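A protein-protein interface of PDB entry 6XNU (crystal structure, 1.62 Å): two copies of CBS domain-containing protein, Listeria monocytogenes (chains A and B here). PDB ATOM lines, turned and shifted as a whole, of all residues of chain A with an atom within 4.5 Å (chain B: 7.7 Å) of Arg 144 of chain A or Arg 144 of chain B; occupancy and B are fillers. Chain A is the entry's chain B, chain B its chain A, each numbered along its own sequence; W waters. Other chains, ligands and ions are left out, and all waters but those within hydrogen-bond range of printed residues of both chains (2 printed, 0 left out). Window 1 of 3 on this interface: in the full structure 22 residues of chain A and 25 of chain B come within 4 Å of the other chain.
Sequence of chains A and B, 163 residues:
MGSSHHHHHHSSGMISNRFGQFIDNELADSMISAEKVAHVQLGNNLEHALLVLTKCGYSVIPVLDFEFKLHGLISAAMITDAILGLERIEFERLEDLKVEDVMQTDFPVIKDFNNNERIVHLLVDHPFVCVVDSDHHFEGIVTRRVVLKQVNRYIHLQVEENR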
ATOM      1  N   LEU A 123     -22.952 -19.670 -19.484  1.00  0.00           N
ATOM      2  CA  LEU A 123     -22.633 -21.073 -19.248  1.00  0.00           C
ATOM      3  C   LEU A 123     -21.246 -21.263 -18.654  1.00  0.00           C
ATOM      4  O   LEU A 123     -20.910 -22.384 -18.240  1.00  0.00           O
ATOM      5  CB  LEU A 123     -22.765 -21.860 -20.549  1.00  0.00           C
ATOM      6  CG  LEU A 123     -24.196 -22.077 -21.039  1.00  0.00           C
ATOM      7  CD1 LEU A 123     -24.219 -22.698 -22.433  1.00  0.00           C
ATOM      8  CD2 LEU A 123     -24.948 -22.960 -20.021  1.00  0.00           C
ATOM      9  N   VAL A 124     -20.432 -20.210 -18.599  1.00  0.00           N
ATOM     10  CA  VAL A 124     -19.161 -20.320 -17.890  1.00  0.00           C
ATOM     11  C   VAL A 124     -19.407 -20.576 -16.407  1.00  0.00           C
ATOM     12  O   VAL A 124     -18.809 -21.479 -15.810  1.00  0.00           O
ATOM     13  CB  VAL A 124     -18.301 -19.067 -18.116  1.00  0.00           C
ATOM     14  CG1 VAL A 124     -17.083 -19.095 -17.200  1.00  0.00           C
ATOM     15  CG2 VAL A 124     -17.890 -18.969 -19.592  1.00  0.00           C
ATOM     16  N   ASP A 125     -20.312 -19.818 -15.793  1.00  0.00           N
ATOM     17  CA  ASP A 125     -20.557 -19.933 -14.362  1.00  0.00           C
ATOM     18  C   ASP A 125     -21.850 -20.650 -14.018  1.00  0.00           C
ATOM     19  O   ASP A 125     -22.155 -20.798 -12.824  1.00  0.00           O
ATOM     20  CB  ASP A 125     -20.544 -18.548 -13.706  1.00  0.00           C
ATOM     21  CG  ASP A 125     -19.150 -17.939 -13.661  1.00  0.00           C
ATOM     22  OD1 ASP A 125     -18.170 -18.665 -13.925  1.00  0.00           O
ATOM     23  OD2 ASP A 125     -19.028 -16.735 -13.354  1.00  0.00           O
ATOM     24  N   HIS A 126     -22.617 -21.110 -15.007  1.00  0.00           N
ATOM     25  CA  HIS A 126     -23.875 -21.800 -14.740  1.00  0.00           C
ATOM     26  C   HIS A 126     -23.930 -23.101 -15.541  1.00  0.00           C
ATOM     27  O   HIS A 126     -23.749 -23.073 -16.766  1.00  0.00           O
ATOM     28  CB  HIS A 126     -25.080 -20.922 -15.113  1.00  0.00           C
ATOM     29  CG  HIS A 126     -25.203 -19.679 -14.294  1.00  0.00           C
ATOM     30  ND1 HIS A 126     -24.681 -18.470 -14.694  1.00  0.00           N
ATOM     31  CD2 HIS A 126     -25.795 -19.457 -13.096  1.00  0.00           C
ATOM     32  CE1 HIS A 126     -24.950 -17.552 -13.782  1.00  0.00           C
ATOM     33  NE2 HIS A 126     -25.625 -18.126 -12.804  1.00  0.00           N
ATOM     34  N   PRO A 127     -24.208 -24.240 -14.909  1.00  0.00           N
ATOM     35  CA  PRO A 127     -24.291 -25.490 -15.686  1.00  0.00           C
ATOM     36  C   PRO A 127     -25.451 -25.508 -16.659  1.00  0.00           C
ATOM     37  O   PRO A 127     -25.401 -26.247 -17.654  1.00  0.00           O
ATOM     38  CB  PRO A 127     -24.452 -26.571 -14.607  1.00  0.00           C
ATOM     39  CG  PRO A 127     -24.043 -25.915 -13.332  1.00  0.00           C
ATOM     40  CD  PRO A 127     -24.383 -24.471 -13.465  1.00  0.00           C
ATOM     41  N   THR A 143     -27.929 -26.290 -21.688  1.00  0.00           N
ATOM     42  CA  THR A 143     -26.883 -26.779 -20.792  1.00  0.00           C
ATOM     43  C   THR A 143     -25.510 -26.669 -21.450  1.00  0.00           C
ATOM     44  O   THR A 143     -25.383 -26.400 -22.643  1.00  0.00           O
ATOM     45  CB  THR A 143     -27.138 -28.232 -20.360  1.00  0.00           C
ATOM     46  OG1 THR A 143     -26.640 -29.137 -21.357  1.00  0.00           O
ATOM     47  CG2 THR A 143     -28.627 -28.479 -20.146  1.00  0.00           C
ATOM     48  N   ARG A 144     -24.468 -26.918 -20.648  1.00  0.00           N
ATOM     49  CA  ARG A 144     -23.097 -26.883 -21.154  1.00  0.00           C
ATOM     50  C   ARG A 144     -22.793 -28.004 -22.139  1.00  0.00           C
ATOM     51  O   ARG A 144     -21.807 -27.901 -22.878  1.00  0.00           O
ATOM     52  CB  ARG A 144     -22.090 -26.981 -20.004  1.00  0.00           C
ATOM     53  CG  ARG A 144     -22.036 -25.793 -19.067  1.00  0.00           C
ATOM     54  CD  ARG A 144     -21.004 -26.068 -17.975  1.00  0.00           C
ATOM     55  NE  ARG A 144     -20.751 -24.913 -17.123  1.00  0.00           N
ATOM     56  CZ  ARG A 144     -20.360 -24.998 -15.857  1.00  0.00           C
ATOM     57  NH1 ARG A 144     -20.138 -23.896 -15.152  1.00  0.00           N
ATOM     58  NH2 ARG A 144     -20.196 -26.196 -15.295  1.00  0.00           N
ATOM     59  N   ARG A 145     -23.593 -29.074 -22.162  1.00  0.00           N
ATOM     60  CA  ARG A 145     -23.188 -30.285 -22.875  1.00  0.00           C
ATOM     61  C   ARG A 145     -23.062 -30.056 -24.380  1.00  0.00           C
ATOM     62  O   ARG A 145     -22.172 -30.623 -25.031  1.00  0.00           O
ATOM     63  CB  ARG A 145     -24.173 -31.419 -22.589  1.00  0.00           C
ATOM     64  CG  ARG A 145     -23.789 -32.711 -23.287  1.00  0.00           C
ATOM     65  CD  ARG A 145     -24.616 -33.885 -22.812  1.00  0.00           C
ATOM     66  NE  ARG A 145     -24.240 -35.098 -23.523  1.00  0.00           N
ATOM     67  CZ  ARG A 145     -24.720 -35.437 -24.712  1.00  0.00           C
ATOM     68  NH1 ARG A 145     -25.597 -34.652 -25.317  1.00  0.00           N
ATOM     69  NH2 ARG A 145     -24.323 -36.558 -25.297  1.00  0.00           N
ATOM     70  N   VAL A 146     -23.940 -29.235 -24.954  1.00  0.00           N
ATOM     71  CA  VAL A 146     -23.894 -29.005 -26.398  1.00  0.00           C
ATOM     72  C   VAL A 146     -22.575 -28.361 -26.796  1.00  0.00           C
ATOM     73  O   VAL A 146     -22.005 -28.681 -27.848  1.00  0.00           O
ATOM     74  CB  VAL A 146     -25.087 -28.143 -26.850  1.00  0.00           C
ATOM     75  CG1 VAL A 146     -25.140 -26.838 -26.062  1.00  0.00           C
ATOM     76  CG2 VAL A 146     -24.989 -27.875 -28.349  1.00  0.00           C
ATOM     77  N   VAL A 147     -22.068 -27.443 -25.965  1.00  0.00           N
ATOM     78  CA  VAL A 147     -20.774 -26.822 -26.243  1.00  0.00           C
ATOM     79  C   VAL A 147     -19.667 -27.861 -26.185  1.00  0.00           C
ATOM     80  O   VAL A 147     -18.768 -27.882 -27.032  1.00  0.00           O
ATOM     81  CB  VAL A 147     -20.515 -25.664 -25.261  1.00  0.00           C
ATOM     82  CG1 VAL A 147     -19.165 -25.010 -25.540  1.00  0.00           C
ATOM     83  CG2 VAL A 147     -21.639 -24.648 -25.328  1.00  0.00           C
ATOM     84  N   LEU A 148     -19.704 -28.736 -25.177  1.00  0.00           N
ATOM     85  CA  LEU A 148     -18.711 -29.798 -25.096  1.00  0.00           C
ATOM     86  C   LEU A 148     -18.776 -30.701 -26.322  1.00  0.00           C
ATOM     87  O   LEU A 148     -17.738 -31.127 -26.849  1.00  0.00           O
ATOM     88  CB  LEU A 148     -18.917 -30.607 -23.811  1.00  0.00           C
ATOM     89  CG  LEU A 148     -18.063 -30.150 -22.631  1.00  0.00           C
ATOM     90  CD1 LEU A 148     -16.593 -30.396 -22.914  1.00  0.00           C
ATOM     91  CD2 LEU A 148     -18.307 -28.674 -22.348  1.00  0.00           C
ATOM     92  N   LEU B  27      -5.747 -27.233 -18.998  1.00  0.00           N
ATOM     93  CA  LEU B  27      -6.594 -28.254 -18.387  1.00  0.00           C
ATOM     94  C   LEU B  27      -6.018 -28.704 -17.054  1.00  0.00           C
ATOM     95  O   LEU B  27      -6.751 -28.824 -16.069  1.00  0.00           O
ATOM     96  CB  LEU B  27      -6.760 -29.454 -19.323  1.00  0.00           C
ATOM     97  CG  LEU B  27      -7.773 -29.340 -20.461  1.00  0.00           C
ATOM     98  CD1 LEU B  27      -7.918 -30.683 -21.155  1.00  0.00           C
ATOM     99  CD2 LEU B  27      -9.115 -28.863 -19.944  1.00  0.00           C
ATOM    100  N   VAL B 120     -11.585 -33.848 -22.918  1.00  0.00           N
ATOM    101  CA  VAL B 120     -12.742 -33.145 -23.467  1.00  0.00           C
ATOM    102  C   VAL B 120     -13.840 -34.134 -23.838  1.00  0.00           C
ATOM    103  O   VAL B 120     -15.031 -33.875 -23.624  1.00  0.00           O
ATOM    104  CB  VAL B 120     -12.313 -32.285 -24.669  1.00  0.00           C
ATOM    105  CG1 VAL B 120     -13.525 -31.637 -25.315  1.00  0.00           C
ATOM    106  CG2 VAL B 120     -11.314 -31.229 -24.221  1.00  0.00           C
ATOM    107  N   LEU B 122     -14.480 -37.055 -22.398  1.00  0.00           N
ATOM    108  CA  LEU B 122     -15.152 -37.512 -21.182  1.00  0.00           C
ATOM    109  C   LEU B 122     -16.122 -36.458 -20.661  1.00  0.00           C
ATOM    110  O   LEU B 122     -17.203 -36.789 -20.152  1.00  0.00           O
ATOM    111  CB  LEU B 122     -14.119 -37.859 -20.114  1.00  0.00           C
ATOM    112  CG  LEU B 122     -13.282 -39.103 -20.403  1.00  0.00           C
ATOM    113  CD1 LEU B 122     -12.219 -39.274 -19.341  1.00  0.00           C
ATOM    114  CD2 LEU B 122     -14.174 -40.331 -20.481  1.00  0.00           C
ATOM    115  N   LEU B 123     -15.756 -35.182 -20.786  1.00  0.00           N
ATOM    116  CA  LEU B 123     -16.586 -34.110 -20.257  1.00  0.00           C
ATOM    117  C   LEU B 123     -17.880 -33.931 -21.041  1.00  0.00           C
ATOM    118  O   LEU B 123     -18.754 -33.184 -20.592  1.00  0.00           O
ATOM    119  CB  LEU B 123     -15.786 -32.800 -20.220  1.00  0.00           C
ATOM    120  CG  LEU B 123     -14.665 -32.800 -19.170  1.00  0.00           C
ATOM    121  CD1 LEU B 123     -13.728 -31.606 -19.346  1.00  0.00           C
ATOM    122  CD2 LEU B 123     -15.243 -32.840 -17.759  1.00  0.00           C
ATOM    123  N   VAL B 124     -18.031 -34.613 -22.180  1.00  0.00           N
ATOM    124  CA  VAL B 124     -19.298 -34.571 -22.907  1.00  0.00           C
ATOM    125  C   VAL B 124     -20.417 -35.187 -22.075  1.00  0.00           C
ATOM    126  O   VAL B 124     -21.489 -34.597 -21.908  1.00  0.00           O
ATOM    127  CB  VAL B 124     -19.154 -35.273 -24.267  1.00  0.00           C
ATOM    128  CG1 VAL B 124     -20.516 -35.447 -24.919  1.00  0.00           C
ATOM    129  CG2 VAL B 124     -18.230 -34.470 -25.161  1.00  0.00           C
ATOM    130  N   ASP B 125     -20.192 -36.384 -21.541  1.00  0.00           N
ATOM    131  CA  ASP B 125     -21.233 -37.055 -20.778  1.00  0.00           C
ATOM    132  C   ASP B 125     -20.967 -37.030 -19.281  1.00  0.00           C
ATOM    133  O   ASP B 125     -21.696 -37.673 -18.517  1.00  0.00           O
ATOM    134  CB  ASP B 125     -21.406 -38.491 -21.273  1.00  0.00           C
ATOM    135  CG  ASP B 125     -22.079 -38.555 -22.634  1.00  0.00           C
ATOM    136  OD1 ASP B 125     -23.065 -37.819 -22.856  1.00  0.00           O
ATOM    137  OD2 ASP B 125     -21.613 -39.333 -23.488  1.00  0.00           O
ATOM    138  N   HIS B 126     -19.946 -36.292 -18.843  1.00  0.00           N
ATOM    139  CA  HIS B 126     -19.645 -36.184 -17.424  1.00  0.00           C
ATOM    140  C   HIS B 126     -19.372 -34.731 -17.054  1.00  0.00           C
ATOM    141  O   HIS B 126     -18.446 -34.109 -17.590  1.00  0.00           O
ATOM    142  CB  HIS B 126     -18.456 -37.074 -17.059  1.00  0.00           C
ATOM    143  CG  HIS B 126     -18.647 -38.507 -17.442  1.00  0.00           C
ATOM    144  ND1 HIS B 126     -18.190 -39.025 -18.636  1.00  0.00           N
ATOM    145  CD2 HIS B 126     -19.263 -39.526 -16.798  1.00  0.00           C
ATOM    146  CE1 HIS B 126     -18.512 -40.305 -18.707  1.00  0.00           C
ATOM    147  NE2 HIS B 126     -19.165 -40.633 -17.605  1.00  0.00           N
ATOM    148  N   PRO B 127     -20.176 -34.162 -16.158  1.00  0.00           N
ATOM    149  CA  PRO B 127     -19.932 -32.780 -15.713  1.00  0.00           C
ATOM    150  C   PRO B 127     -18.581 -32.579 -15.054  1.00  0.00           C
ATOM    151  O   PRO B 127     -18.032 -31.474 -15.110  1.00  0.00           O
ATOM    152  CB  PRO B 127     -21.080 -32.533 -14.726  1.00  0.00           C
ATOM    153  CG  PRO B 127     -22.167 -33.440 -15.194  1.00  0.00           C
ATOM    154  CD  PRO B 127     -21.469 -34.682 -15.683  1.00  0.00           C
ATOM    155  N   PHE B 128     -18.047 -33.601 -14.388  1.00  0.00           N
ATOM    156  CA  PHE B 128     -16.672 -33.562 -13.912  1.00  0.00           C
ATOM    157  C   PHE B 128     -16.111 -34.964 -14.001  1.00  0.00           C
ATOM    158  O   PHE B 128     -16.853 -35.948 -14.062  1.00  0.00           O
ATOM    159  CB  PHE B 128     -16.548 -33.048 -12.470  1.00  0.00           C
ATOM    160  CG  PHE B 128     -17.137 -33.978 -11.442  1.00  0.00           C
ATOM    161  CD1 PHE B 128     -18.480 -33.890 -11.111  1.00  0.00           C
ATOM    162  CD2 PHE B 128     -16.352 -34.930 -10.808  1.00  0.00           C
ATOM    163  CE1 PHE B 128     -19.032 -34.742 -10.165  1.00  0.00           C
ATOM    164  CE2 PHE B 128     -16.896 -35.783  -9.870  1.00  0.00           C
ATOM    165  CZ  PHE B 128     -18.233 -35.686  -9.548  1.00  0.00           C
ATOM    166  N   VAL B 129     -14.789 -35.033 -14.002  1.00  0.00           N
ATOM    167  CA  VAL B 129     -14.079 -36.306 -14.013  1.00  0.00           C
ATOM    168  C   VAL B 129     -12.996 -36.273 -12.951  1.00  0.00           C
ATOM    169  O   VAL B 129     -12.254 -35.294 -12.836  1.00  0.00           O
ATOM    170  CB  VAL B 129     -13.482 -36.619 -15.396  1.00  0.00           C
ATOM    171  CG1 VAL B 129     -12.731 -37.951 -15.354  1.00  0.00           C
ATOM    172  CG2 VAL B 129     -14.589 -36.692 -16.422  1.00  0.00           C
ATOM    173  N   VAL B 142     -11.591 -32.426 -12.608  1.00  0.00           N
ATOM    174  CA  VAL B 142     -11.649 -31.494 -13.730  1.00  0.00           C
ATOM    175  C   VAL B 142     -13.116 -31.347 -14.109  1.00  0.00           C
ATOM    176  O   VAL B 142     -13.832 -32.349 -14.190  1.00  0.00           O
ATOM    177  CB  VAL B 142     -10.811 -32.002 -14.920  1.00  0.00           C
ATOM    178  CG1 VAL B 142     -10.974 -31.085 -16.117  1.00  0.00           C
ATOM    179  CG2 VAL B 142      -9.348 -32.099 -14.530  1.00  0.00           C
ATOM    180  N   THR B 143     -13.579 -30.108 -14.324  1.00  0.00           N
ATOM    181  CA  THR B 143     -14.981 -29.889 -14.651  1.00  0.00           C
ATOM    182  C   THR B 143     -15.120 -29.265 -16.037  1.00  0.00           C
ATOM    183  O   THR B 143     -14.142 -28.895 -16.693  1.00  0.00           O
ATOM    184  CB  THR B 143     -15.696 -29.009 -13.604  1.00  0.00           C
ATOM    185  OG1 THR B 143     -15.467 -27.613 -13.862  1.00  0.00           O
ATOM    186  CG2 THR B 143     -15.228 -29.358 -12.180  1.00  0.00           C
ATOM    187  N   ARG B 144     -16.376 -29.153 -16.470  1.00  0.00           N
ATOM    188  CA  ARG B 144     -16.668 -28.577 -17.780  1.00  0.00           C
ATOM    189  C   ARG B 144     -16.345 -27.096 -17.854  1.00  0.00           C
ATOM    190  O   ARG B 144     -16.182 -26.560 -18.966  1.00  0.00           O
ATOM    191  CB  ARG B 144     -18.142 -28.769 -18.104  1.00  0.00           C
ATOM    192  CG  ARG B 144     -18.506 -30.138 -18.590  1.00  0.00           C
ATOM    193  CD  ARG B 144     -20.008 -30.204 -18.744  1.00  0.00           C
ATOM    194  NE  ARG B 144     -20.459 -31.486 -19.274  1.00  0.00           N
ATOM    195  CZ  ARG B 144     -21.694 -31.945 -19.122  1.00  0.00           C
ATOM    196  NH1 ARG B 144     -22.579 -31.218 -18.455  1.00  0.00           N
ATOM    197  NH2 ARG B 144     -22.046 -33.112 -19.643  1.00  0.00           N
ATOM    198  N   ARG B 145     -16.245 -26.415 -16.710  1.00  0.00           N
ATOM    199  CA  ARG B 145     -16.125 -24.959 -16.728  1.00  0.00           C
ATOM    200  C   ARG B 145     -14.887 -24.498 -17.490  1.00  0.00           C
ATOM    201  O   ARG B 145     -14.939 -23.487 -18.200  1.00  0.00           O
ATOM    202  CB  ARG B 145     -16.102 -24.412 -15.303  1.00  0.00           C
ATOM    203  CG  ARG B 145     -15.910 -22.906 -15.240  1.00  0.00           C
ATOM    204  CD  ARG B 145     -16.289 -22.395 -13.868  1.00  0.00           C
ATOM    205  NE  ARG B 145     -16.243 -20.939 -13.784  1.00  0.00           N
ATOM    206  CZ  ARG B 145     -15.149 -20.247 -13.499  1.00  0.00           C
ATOM    207  NH1 ARG B 145     -14.004 -20.879 -13.271  1.00  0.00           N
ATOM    208  NH2 ARG B 145     -15.202 -18.922 -13.444  1.00  0.00           N
ATOM    209  N   VAL B 146     -13.761 -25.216 -17.360  1.00  0.00           N
ATOM    210  CA  VAL B 146     -12.542 -24.775 -18.039  1.00  0.00           C
ATOM    211  C   VAL B 146     -12.757 -24.757 -19.550  1.00  0.00           C
ATOM    212  O   VAL B 146     -12.259 -23.866 -20.248  1.00  0.00           O
ATOM    213  CB  VAL B 146     -11.335 -25.657 -17.644  1.00  0.00           C
ATOM    214  CG1 VAL B 146     -11.555 -27.116 -18.031  1.00  0.00           C
ATOM    215  CG2 VAL B 146     -10.063 -25.128 -18.295  1.00  0.00           C
ATOM    216  N   VAL B 147     -13.521 -25.717 -20.077  1.00  0.00           N
ATOM    217  CA  VAL B 147     -13.751 -25.751 -21.522  1.00  0.00           C
ATOM    218  C   VAL B 147     -14.662 -24.602 -21.933  1.00  0.00           C
ATOM    219  O   VAL B 147     -14.443 -23.953 -22.966  1.00  0.00           O
ATOM    220  CB  VAL B 147     -14.332 -27.112 -21.945  1.00  0.00           C
ATOM    221  CG1 VAL B 147     -14.620 -27.122 -23.452  1.00  0.00           C
ATOM    222  CG2 VAL B 147     -13.359 -28.261 -21.558  1.00  0.00           C
ATOM    223  N   LEU B 148     -15.683 -24.310 -21.121  1.00  0.00           N
ATOM    224  CA  LEU B 148     -16.535 -23.161 -21.417  1.00  0.00           C
ATOM    225  C   LEU B 148     -15.736 -21.863 -21.384  1.00  0.00           C
ATOM    226  O   LEU B 148     -15.973 -20.963 -22.195  1.00  0.00           O
ATOM    227  CB  LEU B 148     -17.705 -23.095 -20.432  1.00  0.00           C
ATOM    228  CG  LEU B 148     -19.003 -23.741 -20.912  1.00  0.00           C
ATOM    229  CD1 LEU B 148     -19.641 -22.938 -22.067  1.00  0.00           C
ATOM    230  CD2 LEU B 148     -18.771 -25.173 -21.333  1.00  0.00           C
ATOM    231  N   LYS B 149     -14.787 -21.744 -20.448  1.00  0.00           N
ATOM    232  CA  LYS B 149     -13.927 -20.565 -20.418  1.00  0.00           C
ATOM    233  C   LYS B 149     -13.134 -20.452 -21.707  1.00  0.00           C
ATOM    234  O   LYS B 149     -12.985 -19.357 -22.265  1.00  0.00           O
ATOM    235  CB  LYS B 149     -12.969 -20.630 -19.228  1.00  0.00           C
ATOM    236  CG  LYS B 149     -13.597 -20.216 -17.911  1.00  0.00           C
ATOM    237  CD  LYS B 149     -12.614 -20.379 -16.755  1.00  0.00           C
ATOM    238  CE  LYS B 149     -11.453 -19.396 -16.837  1.00  0.00           C
ATOM    239  NZ  LYS B 149     -10.429 -19.672 -15.771  1.00  0.00           N
ATOM    240  N   GLN B 150     -12.629 -21.582 -22.200  1.00  0.00           N
ATOM    241  CA  GLN B 150     -11.863 -21.558 -23.442  1.00  0.00           C
ATOM    242  C   GLN B 150     -12.744 -21.191 -24.633  1.00  0.00           C
ATOM    243  O   GLN B 150     -12.307 -20.448 -25.526  1.00  0.00           O
ATOM    244  CB  GLN B 150     -11.192 -22.912 -23.647  1.00  0.00           C
ATOM    245  CG  GLN B 150     -10.089 -23.161 -22.633  1.00  0.00           C
ATOM    246  CD  GLN B 150      -9.536 -24.576 -22.711  1.00  0.00           C
ATOM    247  OE1 GLN B 150     -10.211 -25.492 -23.195  1.00  0.00           O
ATOM    248  NE2 GLN B 150      -8.306 -24.764 -22.230  1.00  0.00           N
ATOM    249  N   VAL B 151     -13.971 -21.714 -24.676  1.00  0.00           N
ATOM    250  CA  VAL B 151     -14.875 -21.387 -25.780  1.00  0.00           C
ATOM    251  C   VAL B 151     -15.240 -19.907 -25.747  1.00  0.00           C
ATOM    252  O   VAL B 151     -15.246 -19.220 -26.783  1.00  0.00           O
ATOM    253  CB  VAL B 151     -16.124 -22.284 -25.713  1.00  0.00           C
ATOM    254  CG1 VAL B 151     -17.188 -21.792 -26.684  1.00  0.00           C
ATOM    255  CG2 VAL B 151     -15.750 -23.719 -26.033  1.00  0.00           C
HETATM  256  O   HOH W   1     -19.118 -29.264 -14.731  1.00  0.00           O
HETATM  257  O   HOH W   2     -24.557 -28.720 -17.951  1.00  0.00           O
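The backbone carbonyl oxygen of Val 124 of chain A lies close to the guanidinium group of Arg 145 of chain B, 3.3 Å away. OD1 of Asp 125 of chain A is in salt-bridge range of NE of Arg 145 of chain B. The backbone carbonyl oxygen (O) of Val 124 of chain B lies within hydrogen-bond range of the guanidinium group (NE) of Arg 145 of chain A (3.2 Å). NH2 of Arg 145 of chain A is in salt-bridge range of OD1 of Asp 125 of chain B (3.0 Å).
NH1 of Arg 144 of chain A lies within hydrogen-bond range of O of Val 124 of chain A, at 2.8 Å. The backbone carbonyl oxygen (O) of Leu 123 of chain A is in hydrogen-bond range of the guanidinium group (NE) of Arg 144 of chain A. The backbone carbonyl oxygen (O) of Val 124 of chain B is in hydrogen-bond range of the guanidinium group (NH2) of Arg 144 of chain B (2.8 Å). The backbone NH (N) of Arg 145 of chain A sits at hydrogen-bond distance from the side-chain hydroxyl (OG1) of Thr 143 of chain A. The backbone NH (N) of Arg 144 of chain B lies within hydrogen-bond range of the backbone carbonyl oxygen (O) of Pro 127 of chain B. The side-chain hydroxyl (OG1) of Thr 143 of chain B sits close to the backbone NH (N) of Arg 145 of chain B.
Of the 20 printed residues of chain B, 10 touch a printed residue of chain A. Hydrophobic or aromatic side chains of chain B within 4 Å of the printed part of chain A: Leu 123, Val 124, Val 147, Leu 148 and Val 151. Along chain B the printed residues that touch a printed residue of chain A span positions 120 to 151. Hydrophobic or aromatic side chains of chain A within 4 Å of the printed part of chain B: Leu 123, Val 124, Val 147 and Leu 148. Along chain A the printed residues that touch a printed residue of chain B span positions 123 to 148. Among the printed residues, 14 pairs touch across the chains.
Among the printed residues, merely in contact across the chains: Leu 123 of chain A with Leu 148 of chain B, Val 124 of chain A with Leu 148 of chain B, Val 124 of chain A with Lys 149 of chain B, Arg 144 of chain A with Arg 144 of chain B, Val 147 of chain A with Val 151 of chain B, Leu 148 of chain A with Val 120 of chain B, Leu 148 of chain A with Leu 123 of chain B, Leu 148 of chain A with Val 124 of chain B, Leu 148 of chain A with Val 147 of chain B and Leu 148 of chain A with Leu 148 of chain B.
Water W1 lies within hydrogen-bond range of O of Pro 127 of chain B, N of Arg 144 of chain B and NH2 of Arg 144 of chain A. Water W2 lies within hydrogen-bond range of the backbone carbonyl oxygen of Pro 127 of chain A (2.6 Å), the guanidinium group of Arg 144 of chain B (3.2 Å) and the backbone NH of Arg 144 of chain A (3.2 Å).
Leu 123 of chain A touches Leu 148 of chain B, and with the chains exchanged Leu 148 of chain A touches Leu 123 of chain B. Arg 144 of chain A touches its own counterpart, Arg 144 of chain B. Leu 148 of chain A touches Val 147 of chain B, but with the chains exchanged Val 147 of chain A does not touch Leu 148 of chain B (4.1 Å). Leu 148 of chain A touches its own counterpart, Leu 148 of chain B. Positions printed for both chains: 123, 124, 125, 126, 127, 143, 144, 145, 146, 147 and 148. Of the 14 pairs that touch across the chains among the printed residues, 10 have their exchanged pair printed and touching as well.
Of the printed residues of chain A, Arg 144 of chain B touches Arg 144 (3.9 Å). Of the printed residues of chain B, Asp 125 of chain A touches Arg 145 (3.0 Å). Of the printed residues of chain A, Val 151 of chain B touches Val 147 (3.7 Å). Of the printed residues of chain A, Leu 148 of chain B touches Leu 123, Val 124 and Leu 148. Printed residues of chain B within 4 Å of Val 147 of chain A: Val 151. Thr 143 of chain B touches none of the printed residues of chain A. Thr 143 of chain A touches none of the printed residues of chain B. The nearest printed residue of chain B that does not touch Arg 144 of chain A is Leu 148 of chain B (4.01 Å).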
